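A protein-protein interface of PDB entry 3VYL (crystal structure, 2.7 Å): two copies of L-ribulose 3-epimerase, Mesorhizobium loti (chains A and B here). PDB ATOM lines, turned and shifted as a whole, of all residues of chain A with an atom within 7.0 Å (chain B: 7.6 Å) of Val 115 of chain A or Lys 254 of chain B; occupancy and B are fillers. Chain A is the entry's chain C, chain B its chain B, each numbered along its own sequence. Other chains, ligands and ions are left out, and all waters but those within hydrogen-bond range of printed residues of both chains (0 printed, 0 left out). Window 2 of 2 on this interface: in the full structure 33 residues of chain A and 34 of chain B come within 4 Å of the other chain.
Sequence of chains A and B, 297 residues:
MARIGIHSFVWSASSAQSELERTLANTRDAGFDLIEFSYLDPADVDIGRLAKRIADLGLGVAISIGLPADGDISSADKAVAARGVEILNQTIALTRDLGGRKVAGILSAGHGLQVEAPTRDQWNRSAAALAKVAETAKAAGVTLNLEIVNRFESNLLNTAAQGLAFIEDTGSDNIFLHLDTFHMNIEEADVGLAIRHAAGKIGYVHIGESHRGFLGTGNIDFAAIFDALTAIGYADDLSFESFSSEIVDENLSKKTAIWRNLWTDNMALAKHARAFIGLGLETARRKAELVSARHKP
Of chain B, only Lys 254 comes within 4 Å of Val 115 of chain A. Of the printed residues of chain B, Asn 155 of chain A touches Trp 259 (3.5 Å). Of chain A, only Leu 113 and Val 115 come within 4 Å of Lys 254 of chain B. Of the printed residues of chain A, Lys 255 of chain B touches Phe 152. The nearest printed residue of chain A that does not touch Trp 259 of chain B is Leu 113 of chain A (4.3 Å).
Among the printed residues, pairs that only touch across the chains: Leu 113 of chain A with Lys 254 of chain B, Gln 114 of chain A with Trp 259 of chain B, Val 115 of chain A with Lys 254 of chain B, Glu 116 of chain A with Trp 259 of chain B, Ala 117 of chain A with Trp 259 of chain B, Phe 152 of chain A with Lys 255 of chain B, Phe 152 of chain A with Thr 256 of chain B and Asn 155 of chain A with Trp 259 of chain B.
The side-chain carboxylate of Glu 250 of chain B lies within salt-bridge range of the side-chain amino group of Lys 254 of chain B (3.2 Å). The backbone carbonyl oxygen of Leu 252 of chain B lies within hydrogen-bond range of the side-chain hydroxyl of Thr 256 of chain B (2.8 Å). The backbone NH (N) of Leu 113 of chain A is in hydrogen-bond range of the backbone carbonyl oxygen (O) of Phe 152 of chain A. The side-chain amide oxygen of Gln 114 of chain A lies close to the backbone carbonyl oxygen of Gly 112 of chain A (3.2 Å). The backbone carbonyl oxygen of Glu 116 of chain A is in hydrogen-bond range of the side-chain amide nitrogen of Asn 155 of chain A.
No position is printed for both chains. Of the 8 pairs that touch across the chains among the printed residues, none has its exchanged pair printed and touching as well.
Hydrophobic or aromatic side chains of chain B that line the printed part of chain A: Trp 259. Hydrophobic or aromatic side chains of chain A within 4 Å of the printed part of chain B: Leu 113 and Phe 152. Among the printed residues, no Asp or Glu carboxylate lies within 4 Å of a Lys or Arg side-chain nitrogen of the other chain.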
ATOM      1  N   GLY A 112      18.398  10.880  15.125  1.00  0.00           N
ATOM      2  CA  GLY A 112      19.229  11.209  16.295  1.00  0.00           C
ATOM      3  C   GLY A 112      19.197  12.687  16.628  1.00  0.00           C
ATOM      4  O   GLY A 112      18.447  13.442  16.002  1.00  0.00           O
ATOM      5  N   LEU A 113      20.003  13.102  17.611  1.00  0.00           N
ATOM      6  CA  LEU A 113      20.104  14.525  17.977  1.00  0.00           C
ATOM      7  C   LEU A 113      21.080  15.316  17.096  1.00  0.00           C
ATOM      8  O   LEU A 113      22.273  15.422  17.403  1.00  0.00           O
ATOM      9  CB  LEU A 113      20.426  14.723  19.472  1.00  0.00           C
ATOM     10  CG  LEU A 113      20.760  16.130  20.009  1.00  0.00           C
ATOM     11  CD1 LEU A 113      19.762  17.189  19.575  1.00  0.00           C
ATOM     12  CD2 LEU A 113      20.894  16.117  21.519  1.00  0.00           C
ATOM     13  N   GLN A 114      20.527  15.899  16.028  1.00  0.00           N
ATOM     14  CA  GLN A 114      21.262  16.701  15.065  1.00  0.00           C
ATOM     15  C   GLN A 114      21.984  17.845  15.739  1.00  0.00           C
ATOM     16  O   GLN A 114      21.522  18.362  16.751  1.00  0.00           O
ATOM     17  CB  GLN A 114      20.311  17.269  14.015  1.00  0.00           C
ATOM     18  CG  GLN A 114      19.514  16.238  13.229  1.00  0.00           C
ATOM     19  CD  GLN A 114      20.331  15.017  12.855  1.00  0.00           C
ATOM     20  OE1 GLN A 114      19.993  13.898  13.237  1.00  0.00           O
ATOM     21  NE2 GLN A 114      21.412  15.227  12.109  1.00  0.00           N
ATOM     22  N   VAL A 115      23.126  18.233  15.178  1.00  0.00           N
ATOM     23  CA  VAL A 115      23.888  19.371  15.701  1.00  0.00           C
ATOM     24  C   VAL A 115      23.702  20.565  14.779  1.00  0.00           C
ATOM     25  O   VAL A 115      24.469  21.521  14.821  1.00  0.00           O
ATOM     26  CB  VAL A 115      25.390  19.041  15.910  1.00  0.00           C
ATOM     27  CG1 VAL A 115      25.584  18.208  17.176  1.00  0.00           C
ATOM     28  CG2 VAL A 115      25.974  18.333  14.697  1.00  0.00           C
ATOM     29  N   GLU A 116      22.646  20.504  13.973  1.00  0.00           N
ATOM     30  CA  GLU A 116      22.429  21.435  12.870  1.00  0.00           C
ATOM     31  C   GLU A 116      20.951  21.805  12.787  1.00  0.00           C
ATOM     32  O   GLU A 116      20.086  20.917  12.754  1.00  0.00           O
ATOM     33  CB  GLU A 116      22.847  20.769  11.550  1.00  0.00           C
ATOM     34  CG  GLU A 116      23.501  21.687  10.538  1.00  0.00           C
ATOM     35  CD  GLU A 116      24.982  21.876  10.815  1.00  0.00           C
ATOM     36  OE1 GLU A 116      25.328  22.834  11.545  1.00  0.00           O
ATOM     37  OE2 GLU A 116      25.797  21.059  10.319  1.00  0.00           O
ATOM     38  N   ALA A 117      20.661  23.103  12.751  1.00  0.00           N
ATOM     39  CA  ALA A 117      19.305  23.575  12.462  1.00  0.00           C
ATOM     40  C   ALA A 117      18.929  23.211  11.024  1.00  0.00           C
ATOM     41  O   ALA A 117      19.765  23.281  10.129  1.00  0.00           O
ATOM     42  CB  ALA A 117      19.213  25.077  12.670  1.00  0.00           C
ATOM     43  N   PHE A 152      14.538  16.042  19.543  1.00  0.00           N
ATOM     44  CA  PHE A 152      15.792  15.345  19.814  1.00  0.00           C
ATOM     45  C   PHE A 152      16.021  14.103  18.951  1.00  0.00           C
ATOM     46  O   PHE A 152      17.061  13.470  19.060  1.00  0.00           O
ATOM     47  CB  PHE A 152      15.871  14.944  21.275  1.00  0.00           C
ATOM     48  CG  PHE A 152      15.666  16.078  22.237  1.00  0.00           C
ATOM     49  CD1 PHE A 152      16.717  16.937  22.560  1.00  0.00           C
ATOM     50  CD2 PHE A 152      14.438  16.264  22.851  1.00  0.00           C
ATOM     51  CE1 PHE A 152      16.533  17.973  23.464  1.00  0.00           C
ATOM     52  CE2 PHE A 152      14.245  17.309  23.755  1.00  0.00           C
ATOM     53  CZ  PHE A 152      15.294  18.159  24.066  1.00  0.00           C
ATOM     54  N   ASN A 155      15.544  16.675  13.179  1.00  0.00           N
ATOM     55  CA  ASN A 155      15.372  18.101  13.099  1.00  0.00           C
ATOM     56  C   ASN A 155      14.503  18.571  11.981  1.00  0.00           C
ATOM     57  O   ASN A 155      14.292  19.737  11.816  1.00  0.00           O
ATOM     58  CB  ASN A 155      16.712  18.769  12.971  1.00  0.00           C
ATOM     59  CG  ASN A 155      17.326  18.578  11.625  1.00  0.00           C
ATOM     60  OD1 ASN A 155      16.749  17.989  10.763  1.00  0.00           O
ATOM     61  ND2 ASN A 155      18.492  19.087  11.451  1.00  0.00           N
ATOM     62  N   SER B 245      15.250  30.416  18.877  1.00  0.00           N
ATOM     63  CA  SER B 245      16.577  30.188  18.290  1.00  0.00           C
ATOM     64  C   SER B 245      17.144  31.447  17.630  1.00  0.00           C
ATOM     65  O   SER B 245      18.357  31.576  17.448  1.00  0.00           O
ATOM     66  CB  SER B 245      16.501  29.068  17.259  1.00  0.00           C
ATOM     67  OG  SER B 245      15.669  29.456  16.179  1.00  0.00           O
ATOM     68  N   VAL B 248      18.269  32.951  21.438  1.00  0.00           N
ATOM     69  CA  VAL B 248      19.256  32.278  22.300  1.00  0.00           C
ATOM     70  C   VAL B 248      20.551  31.898  21.573  1.00  0.00           C
ATOM     71  O   VAL B 248      20.577  31.779  20.349  1.00  0.00           O
ATOM     72  CB  VAL B 248      18.668  31.049  23.057  1.00  0.00           C
ATOM     73  CG1 VAL B 248      17.482  31.461  23.921  1.00  0.00           C
ATOM     74  CG2 VAL B 248      18.299  29.923  22.095  1.00  0.00           C
ATOM     75  N   ASP B 249      21.618  31.721  22.352  1.00  0.00           N
ATOM     76  CA  ASP B 249      22.914  31.273  21.852  1.00  0.00           C
ATOM     77  C   ASP B 249      22.733  29.955  21.126  1.00  0.00           C
ATOM     78  O   ASP B 249      21.990  29.084  21.590  1.00  0.00           O
ATOM     79  CB  ASP B 249      23.890  31.082  23.019  1.00  0.00           C
ATOM     80  CG  ASP B 249      25.351  30.943  22.566  1.00  0.00           C
ATOM     81  OD1 ASP B 249      25.647  31.020  21.350  1.00  0.00           O
ATOM     82  OD2 ASP B 249      26.221  30.753  23.447  1.00  0.00           O
ATOM     83  N   GLU B 250      23.419  29.809  19.995  1.00  0.00           N
ATOM     84  CA  GLU B 250      23.370  28.577  19.205  1.00  0.00           C
ATOM     85  C   GLU B 250      23.767  27.311  19.992  1.00  0.00           C
ATOM     86  O   GLU B 250      23.368  26.202  19.625  1.00  0.00           O
ATOM     87  CB  GLU B 250      24.192  28.712  17.915  1.00  0.00           C
ATOM     88  CG  GLU B 250      25.687  28.876  18.132  1.00  0.00           C
ATOM     89  CD  GLU B 250      26.497  28.215  17.035  1.00  0.00           C
ATOM     90  OE1 GLU B 250      27.085  27.146  17.310  1.00  0.00           O
ATOM     91  OE2 GLU B 250      26.534  28.749  15.902  1.00  0.00           O
ATOM     92  N   ASN B 251      24.535  27.491  21.070  1.00  0.00           N
ATOM     93  CA  ASN B 251      24.900  26.409  21.986  1.00  0.00           C
ATOM     94  C   ASN B 251      23.681  25.724  22.634  1.00  0.00           C
ATOM     95  O   ASN B 251      23.443  24.527  22.420  1.00  0.00           O
ATOM     96  CB  ASN B 251      25.860  26.935  23.062  1.00  0.00           C
ATOM     97  CG  ASN B 251      26.426  25.829  23.940  1.00  0.00           C
ATOM     98  OD1 ASN B 251      26.610  24.693  23.492  1.00  0.00           O
ATOM     99  ND2 ASN B 251      26.715  26.158  25.200  1.00  0.00           N
ATOM    100  N   LEU B 252      22.922  26.495  23.417  1.00  0.00           N
ATOM    101  CA  LEU B 252      21.672  26.044  24.040  1.00  0.00           C
ATOM    102  C   LEU B 252      20.611  25.700  22.987  1.00  0.00           C
ATOM    103  O   LEU B 252      19.774  24.822  23.195  1.00  0.00           O
ATOM    104  CB  LEU B 252      21.134  27.129  24.981  1.00  0.00           C
ATOM    105  CG  LEU B 252      19.786  26.908  25.681  1.00  0.00           C
ATOM    106  CD1 LEU B 252      19.935  25.975  26.874  1.00  0.00           C
ATOM    107  CD2 LEU B 252      19.187  28.235  26.117  1.00  0.00           C
ATOM    108  N   SER B 253      20.659  26.397  21.859  1.00  0.00           N
ATOM    109  CA  SER B 253      19.708  26.191  20.780  1.00  0.00           C
ATOM    110  C   SER B 253      19.843  24.809  20.153  1.00  0.00           C
ATOM    111  O   SER B 253      18.885  24.276  19.579  1.00  0.00           O
ATOM    112  CB  SER B 253      19.902  27.250  19.708  1.00  0.00           C
ATOM    113  OG  SER B 253      18.897  27.136  18.727  1.00  0.00           O
ATOM    114  N   LYS B 254      21.041  24.245  20.251  1.00  0.00           N
ATOM    115  CA  LYS B 254      21.304  22.911  19.739  1.00  0.00           C
ATOM    116  C   LYS B 254      21.167  21.891  20.859  1.00  0.00           C
ATOM    117  O   LYS B 254      20.860  20.727  20.621  1.00  0.00           O
ATOM    118  CB  LYS B 254      22.697  22.840  19.109  1.00  0.00           C
ATOM    119  CG  LYS B 254      22.787  23.451  17.715  1.00  0.00           C
ATOM    120  CD  LYS B 254      24.210  23.386  17.176  1.00  0.00           C
ATOM    121  CE  LYS B 254      25.089  24.515  17.705  1.00  0.00           C
ATOM    122  NZ  LYS B 254      26.498  24.090  17.965  1.00  0.00           N
ATOM    123  N   LYS B 255      21.383  22.340  22.085  1.00  0.00           N
ATOM    124  CA  LYS B 255      21.330  21.455  23.228  1.00  0.00           C
ATOM    125  C   LYS B 255      19.882  21.113  23.604  1.00  0.00           C
ATOM    126  O   LYS B 255      19.596  20.006  24.087  1.00  0.00           O
ATOM    127  CB  LYS B 255      22.084  22.073  24.402  1.00  0.00           C
ATOM    128  CG  LYS B 255      22.953  21.068  25.118  1.00  0.00           C
ATOM    129  CD  LYS B 255      24.216  21.709  25.660  1.00  0.00           C
ATOM    130  CE  LYS B 255      25.384  20.734  25.593  1.00  0.00           C
ATOM    131  NZ  LYS B 255      26.383  21.032  26.656  1.00  0.00           N
ATOM    132  N   THR B 256      18.972  22.057  23.370  1.00  0.00           N
ATOM    133  CA  THR B 256      17.574  21.866  23.721  1.00  0.00           C
ATOM    134  C   THR B 256      16.731  21.758  22.456  1.00  0.00           C
ATOM    135  O   THR B 256      15.496  21.753  22.515  1.00  0.00           O
ATOM    136  CB  THR B 256      17.052  22.995  24.623  1.00  0.00           C
ATOM    137  OG1 THR B 256      17.084  24.239  23.918  1.00  0.00           O
ATOM    138  CG2 THR B 256      17.890  23.112  25.883  1.00  0.00           C
ATOM    139  N   ALA B 257      17.427  21.676  21.326  1.00  0.00           N
ATOM    140  CA  ALA B 257      16.871  21.408  19.990  1.00  0.00           C
ATOM    141  C   ALA B 257      15.716  22.315  19.546  1.00  0.00           C
ATOM    142  O   ALA B 257      14.643  21.847  19.157  1.00  0.00           O
ATOM    143  CB  ALA B 257      16.529  19.929  19.825  1.00  0.00           C
ATOM    144  N   ILE B 258      15.952  23.623  19.586  1.00  0.00           N
ATOM    145  CA  ILE B 258      14.962  24.564  19.088  1.00  0.00           C
ATOM    146  C   ILE B 258      15.142  24.661  17.587  1.00  0.00           C
ATOM    147  O   ILE B 258      16.073  25.310  17.115  1.00  0.00           O
ATOM    148  CB  ILE B 258      15.063  25.963  19.738  1.00  0.00           C
ATOM    149  CG1 ILE B 258      15.241  25.849  21.252  1.00  0.00           C
ATOM    150  CG2 ILE B 258      13.815  26.773  19.430  1.00  0.00           C
ATOM    151  CD1 ILE B 258      15.964  27.030  21.867  1.00  0.00           C
ATOM    152  N   TRP B 259      14.262  23.988  16.851  1.00  0.00           N
ATOM    153  CA  TRP B 259      14.342  23.955  15.393  1.00  0.00           C
ATOM    154  C   TRP B 259      13.313  24.848  14.791  1.00  0.00           C
ATOM    155  O   TRP B 259      13.467  25.306  13.651  1.00  0.00           O
ATOM    156  CB  TRP B 259      14.149  22.536  14.843  1.00  0.00           C
ATOM    157  CG  TRP B 259      15.030  21.463  15.448  1.00  0.00           C
ATOM    158  CD1 TRP B 259      14.641  20.191  15.865  1.00  0.00           C
ATOM    159  CD2 TRP B 259      16.474  21.530  15.739  1.00  0.00           C
ATOM    160  NE1 TRP B 259      15.704  19.490  16.366  1.00  0.00           N
ATOM    161  CE2 TRP B 259      16.834  20.228  16.317  1.00  0.00           C
ATOM    162  CE3 TRP B 259      17.463  22.492  15.585  1.00  0.00           C
ATOM    163  CZ2 TRP B 259      18.138  19.931  16.711  1.00  0.00           C
ATOM    164  CZ3 TRP B 259      18.768  22.179  15.987  1.00  0.00           C
ATOM    165  CH2 TRP B 259      19.095  20.927  16.536  1.00  0.00           C
